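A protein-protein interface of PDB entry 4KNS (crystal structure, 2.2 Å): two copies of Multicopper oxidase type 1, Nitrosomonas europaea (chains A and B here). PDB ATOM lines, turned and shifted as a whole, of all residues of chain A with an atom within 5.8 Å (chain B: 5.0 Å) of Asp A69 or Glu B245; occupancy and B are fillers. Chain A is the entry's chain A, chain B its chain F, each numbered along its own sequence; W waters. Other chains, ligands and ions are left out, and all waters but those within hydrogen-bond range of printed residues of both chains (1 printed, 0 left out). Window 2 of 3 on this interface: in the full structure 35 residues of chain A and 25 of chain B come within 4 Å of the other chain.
Water W1 lies within hydrogen-bond range of the backbone carbonyl oxygen (O) of Leu A68 (2.8 Å) and the backbone carbonyl oxygen (O) of Ala B206 (3.2 Å).
Of the 8 printed residues of chain A, 6 touch a printed residue of chain B.
Hydrophobic or aromatic side chains of chain A that line the printed part of chain B: Val A70, Val A71 and Phe A74.
Along chain A the printed residues that touch a printed residue of chain B span positions 67 to 74.
Hydrophobic or aromatic side chains of chain B within 4 Å of the printed part of chain A: Ala B206, Pro B243 and Ala B247.
Along chain B the printed residues that touch a printed residue of chain A span positions 206 to 247.
Among the printed residues, 11 pairs touch across the chains.
Among the printed residues, pairs that only touch across the chains: Arg A67 with Ala B206 (3.4 Å), Arg A67 with Pro B243 (3.5 Å), Leu A68 with Ala B247 (3.7 Å), Asp A69 with Glu B245 (3.9 Å), Asp A69 with Gly B246 (3.5 Å), Val A70 with Ala B206 (3.6 Å), Val A71 with Ala B247 (3.9 Å) and Phe A74 with Ala B206 (3.6 Å).
The backbone carbonyl oxygen (O) of Ala B206 lies within hydrogen-bond range of the backbone NH (N) of Leu A68 (2.8 Å).
The side-chain carboxylate of Asp A69 sits at hydrogen-bond distance from the backbone NH of Ala B247.
O of Ala B247 is in hydrogen-bond range of N of Val A70 (3.0 Å).
Of the printed residues of chain B, Leu A68 touches Ala B206 (2.8 Å) and Ala B247 (3.7 Å).
Printed residues of chain B within 4 Å of Val A70: Ala B206 (3.6 Å) and Ala B247 (3.0 Å).
Of the printed residues of chain A, Pro B243 touches Arg A67.
Printed residues of chain A within 4 Å of Gly B246: Asp A69 (3.5 Å).
The nearest printed residue of chain A that does not touch Gly B246 is Val A71 (5.8 Å).
No position is printed for both chains.
The backbone NH of Val A71 is in hydrogen-bond range of the side-chain carboxylate of Asp A69, at 3.2 Å.
The side-chain carboxylate (OD2) of Asp A69 lies within hydrogen-bond range of the backbone NH (N) of Glu A72 (3.1 Å).
N of Asp A69 lies within hydrogen-bond range of OD2 of Asp A73, 2.9 Å away.
The side-chain carboxylate of Glu B245 is in hydrogen-bond range of the backbone NH of Asn B270.
N of Phe B268 sits at hydrogen-bond distance from O of Gly B246 (2.8 Å).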
ATOM      1  N   ARG A  67      30.298  24.026  24.686  1.00  0.00           N
ATOM      2  CA  ARG A  67      29.958  25.442  24.557  1.00  0.00           C
ATOM      3  C   ARG A  67      28.827  25.574  23.540  1.00  0.00           C
ATOM      4  O   ARG A  67      29.056  25.489  22.330  1.00  0.00           O
ATOM      5  CB  ARG A  67      31.181  26.259  24.129  1.00  0.00           C
ATOM      6  CG  ARG A  67      32.329  26.239  25.130  1.00  0.00           C
ATOM      7  CD  ARG A  67      33.612  26.771  24.514  1.00  0.00           C
ATOM      8  NE  ARG A  67      33.534  28.204  24.241  1.00  0.00           N
ATOM      9  CZ  ARG A  67      34.234  28.829  23.299  1.00  0.00           C
ATOM     10  NH1 ARG A  67      35.068  28.149  22.518  1.00  0.00           N
ATOM     11  NH2 ARG A  67      34.094  30.137  23.132  1.00  0.00           N
ATOM     12  N   LEU A  68      27.608  25.764  24.044  1.00  0.00           N
ATOM     13  CA  LEU A  68      26.395  25.672  23.228  1.00  0.00           C
ATOM     14  C   LEU A  68      25.297  26.630  23.698  1.00  0.00           C
ATOM     15  O   LEU A  68      25.562  27.594  24.419  1.00  0.00           O
ATOM     16  CB  LEU A  68      25.860  24.229  23.238  1.00  0.00           C
ATOM     17  CG  LEU A  68      26.679  23.093  22.611  1.00  0.00           C
ATOM     18  CD1 LEU A  68      26.161  21.742  23.077  1.00  0.00           C
ATOM     19  CD2 LEU A  68      26.684  23.171  21.090  1.00  0.00           C
ATOM     20  N   ASP A  69      24.065  26.357  23.276  1.00  0.00           N
ATOM     21  CA  ASP A  69      22.898  27.122  23.702  1.00  0.00           C
ATOM     22  C   ASP A  69      22.093  26.316  24.720  1.00  0.00           C
ATOM     23  O   ASP A  69      21.626  25.218  24.424  1.00  0.00           O
ATOM     24  CB  ASP A  69      22.035  27.505  22.491  1.00  0.00           C
ATOM     25  CG  ASP A  69      20.672  28.055  22.884  1.00  0.00           C
ATOM     26  OD1 ASP A  69      20.575  28.788  23.893  1.00  0.00           O
ATOM     27  OD2 ASP A  69      19.691  27.756  22.173  1.00  0.00           O
ATOM     28  N   VAL A  70      21.937  26.875  25.918  1.00  0.00           N
ATOM     29  CA  VAL A  70      21.227  26.202  27.010  1.00  0.00           C
ATOM     30  C   VAL A  70      19.749  25.947  26.684  1.00  0.00           C
ATOM     31  O   VAL A  70      19.211  24.897  27.034  1.00  0.00           O
ATOM     32  CB  VAL A  70      21.387  26.959  28.361  1.00  0.00           C
ATOM     33  CG1 VAL A  70      20.838  28.381  28.280  1.00  0.00           C
ATOM     34  CG2 VAL A  70      20.728  26.192  29.501  1.00  0.00           C
ATOM     35  N   VAL A  71      19.119  26.894  25.991  1.00  0.00           N
ATOM     36  CA  VAL A  71      17.686  26.832  25.698  1.00  0.00           C
ATOM     37  C   VAL A  71      17.330  25.665  24.768  1.00  0.00           C
ATOM     38  O   VAL A  71      16.405  24.902  25.058  1.00  0.00           O
ATOM     39  CB  VAL A  71      17.160  28.173  25.125  1.00  0.00           C
ATOM     40  CG1 VAL A  71      15.661  28.104  24.862  1.00  0.00           C
ATOM     41  CG2 VAL A  71      17.467  29.321  26.076  1.00  0.00           C
ATOM     42  N   GLU A  72      18.072  25.518  23.672  1.00  0.00           N
ATOM     43  CA  GLU A  72      17.759  24.499  22.665  1.00  0.00           C
ATOM     44  C   GLU A  72      18.532  23.188  22.825  1.00  0.00           C
ATOM     45  O   GLU A  72      17.986  22.114  22.581  1.00  0.00           O
ATOM     46  CB  GLU A  72      17.940  25.050  21.244  1.00  0.00           C
ATOM     47  CG  GLU A  72      16.982  26.177  20.864  1.00  0.00           C
ATOM     48  CD  GLU A  72      15.522  25.745  20.786  1.00  0.00           C
ATOM     49  OE1 GLU A  72      15.246  24.547  20.548  1.00  0.00           O
ATOM     50  OE2 GLU A  72      14.643  26.618  20.955  1.00  0.00           O
ATOM     51  N   ASP A  73      19.793  23.273  23.234  1.00  0.00           N
ATOM     52  CA  ASP A  73      20.643  22.084  23.321  1.00  0.00           C
ATOM     53  C   ASP A  73      20.475  21.302  24.621  1.00  0.00           C
ATOM     54  O   ASP A  73      20.505  20.071  24.612  1.00  0.00           O
ATOM     55  CB  ASP A  73      22.113  22.446  23.092  1.00  0.00           C
ATOM     56  CG  ASP A  73      22.350  23.080  21.735  1.00  0.00           C
ATOM     57  OD1 ASP A  73      21.996  22.453  20.712  1.00  0.00           O
ATOM     58  OD2 ASP A  73      22.889  24.207  21.690  1.00  0.00           O
ATOM     59  N   PHE A  74      20.292  22.013  25.732  1.00  0.00           N
ATOM     60  CA  PHE A  74      20.182  21.371  27.044  1.00  0.00           C
ATOM     61  C   PHE A  74      18.730  21.200  27.510  1.00  0.00           C
ATOM     62  O   PHE A  74      18.479  20.941  28.690  1.00  0.00           O
ATOM     63  CB  PHE A  74      20.997  22.135  28.104  1.00  0.00           C
ATOM     64  CG  PHE A  74      22.494  22.103  27.888  1.00  0.00           C
ATOM     65  CD1 PHE A  74      23.073  21.299  26.908  1.00  0.00           C
ATOM     66  CD2 PHE A  74      23.330  22.865  28.699  1.00  0.00           C
ATOM     67  CE1 PHE A  74      24.449  21.273  26.725  1.00  0.00           C
ATOM     68  CE2 PHE A  74      24.708  22.840  28.525  1.00  0.00           C
ATOM     69  CZ  PHE A  74      25.269  22.045  27.536  1.00  0.00           C
ATOM     70  N   PRO B 183      27.914  36.707  19.480  1.00  0.00           N
ATOM     71  CA  PRO B 183      28.867  35.596  19.434  1.00  0.00           C
ATOM     72  C   PRO B 183      30.265  36.081  19.059  1.00  0.00           C
ATOM     73  O   PRO B 183      30.403  36.963  18.210  1.00  0.00           O
ATOM     74  CB  PRO B 183      28.306  34.696  18.329  1.00  0.00           C
ATOM     75  CG  PRO B 183      26.851  35.007  18.288  1.00  0.00           C
ATOM     76  CD  PRO B 183      26.745  36.468  18.612  1.00  0.00           C
ATOM     77  N   ALA B 206      26.238  25.955  29.655  1.00  0.00           N
ATOM     78  CA  ALA B 206      26.439  25.924  28.200  1.00  0.00           C
ATOM     79  C   ALA B 206      27.619  26.791  27.736  1.00  0.00           C
ATOM     80  O   ALA B 206      27.751  27.096  26.547  1.00  0.00           O
ATOM     81  CB  ALA B 206      25.156  26.280  27.450  1.00  0.00           C
ATOM     82  N   PRO B 243      30.782  30.843  21.209  1.00  0.00           N
ATOM     83  CA  PRO B 243      31.083  30.639  19.792  1.00  0.00           C
ATOM     84  C   PRO B 243      29.837  30.671  18.902  1.00  0.00           C
ATOM     85  O   PRO B 243      29.962  30.782  17.679  1.00  0.00           O
ATOM     86  CB  PRO B 243      31.720  29.248  19.770  1.00  0.00           C
ATOM     87  CG  PRO B 243      31.103  28.537  20.923  1.00  0.00           C
ATOM     88  CD  PRO B 243      30.819  29.578  21.971  1.00  0.00           C
ATOM     89  N   VAL B 244      28.656  30.577  19.511  1.00  0.00           N
ATOM     90  CA  VAL B 244      27.393  30.490  18.766  1.00  0.00           C
ATOM     91  C   VAL B 244      26.294  31.392  19.334  1.00  0.00           C
ATOM     92  O   VAL B 244      26.420  31.923  20.442  1.00  0.00           O
ATOM     93  CB  VAL B 244      26.866  29.035  18.689  1.00  0.00           C
ATOM     94  CG1 VAL B 244      27.663  28.223  17.676  1.00  0.00           C
ATOM     95  CG2 VAL B 244      26.880  28.368  20.061  1.00  0.00           C
ATOM     96  N   GLU B 245      25.223  31.562  18.558  1.00  0.00           N
ATOM     97  CA  GLU B 245      24.023  32.259  19.016  1.00  0.00           C
ATOM     98  C   GLU B 245      23.250  31.396  20.009  1.00  0.00           C
ATOM     99  O   GLU B 245      23.366  30.169  19.999  1.00  0.00           O
ATOM    100  CB  GLU B 245      23.116  32.624  17.835  1.00  0.00           C
ATOM    101  CG  GLU B 245      23.562  33.850  17.049  1.00  0.00           C
ATOM    102  CD  GLU B 245      22.507  34.346  16.072  1.00  0.00           C
ATOM    103  OE1 GLU B 245      21.947  33.522  15.316  1.00  0.00           O
ATOM    104  OE2 GLU B 245      22.244  35.568  16.056  1.00  0.00           O
ATOM    105  N   GLY B 246      22.463  32.049  20.862  1.00  0.00           N
ATOM    106  CA  GLY B 246      21.654  31.357  21.858  1.00  0.00           C
ATOM    107  C   GLY B 246      21.737  32.004  23.225  1.00  0.00           C
ATOM    108  O   GLY B 246      21.683  33.230  23.343  1.00  0.00           O
ATOM    109  N   ALA B 247      21.875  31.176  24.258  1.00  0.00           N
ATOM    110  CA  ALA B 247      21.921  31.660  25.636  1.00  0.00           C
ATOM    111  C   ALA B 247      22.858  30.853  26.534  1.00  0.00           C
ATOM    112  O   ALA B 247      23.076  29.657  26.319  1.00  0.00           O
ATOM    113  CB  ALA B 247      20.520  31.685  26.231  1.00  0.00           C
ATOM    114  N   PHE B 268      23.000  35.675  23.499  1.00  0.00           N
ATOM    115  CA  PHE B 268      23.961  35.901  22.426  1.00  0.00           C
ATOM    116  C   PHE B 268      23.251  35.978  21.076  1.00  0.00           C
ATOM    117  O   PHE B 268      22.940  34.954  20.467  1.00  0.00           O
ATOM    118  CB  PHE B 268      25.041  34.810  22.419  1.00  0.00           C
ATOM    119  CG  PHE B 268      25.878  34.774  23.669  1.00  0.00           C
ATOM    120  CD1 PHE B 268      26.966  35.630  23.822  1.00  0.00           C
ATOM    121  CD2 PHE B 268      25.581  33.881  24.695  1.00  0.00           C
ATOM    122  CE1 PHE B 268      27.739  35.596  24.973  1.00  0.00           C
ATOM    123  CE2 PHE B 268      26.351  33.844  25.849  1.00  0.00           C
ATOM    124  CZ  PHE B 268      27.433  34.701  25.988  1.00  0.00           C
ATOM    125  N   THR B 269      22.977  37.201  20.631  1.00  0.00           N
ATOM    126  CA  THR B 269      22.322  37.437  19.341  1.00  0.00           C
ATOM    127  C   THR B 269      23.194  38.319  18.449  1.00  0.00           C
ATOM    128  O   THR B 269      23.943  39.164  18.947  1.00  0.00           O
ATOM    129  CB  THR B 269      20.928  38.090  19.501  1.00  0.00           C
ATOM    130  OG1 THR B 269      21.066  39.408  20.049  1.00  0.00           O
ATOM    131  CG2 THR B 269      20.025  37.255  20.407  1.00  0.00           C
ATOM    132  N   ASN B 270      23.085  38.119  17.136  1.00  0.00           N
ATOM    133  CA  ASN B 270      23.856  38.887  16.153  1.00  0.00           C
ATOM    134  C   ASN B 270      23.532  40.383  16.118  1.00  0.00           C
ATOM    135  O   ASN B 270      24.373  41.193  15.720  1.00  0.00           O
ATOM    136  CB  ASN B 270      23.717  38.277  14.752  1.00  0.00           C
ATOM    137  CG  ASN B 270      24.636  37.087  14.533  1.00  0.00           C
ATOM    138  OD1 ASN B 270      24.284  36.142  13.827  1.00  0.00           O
ATOM    139  ND2 ASN B 270      25.822  37.127  15.135  1.00  0.00           N
HETATM  140  O   HOH W   1      27.994  28.982  23.924  1.00  0.00           O
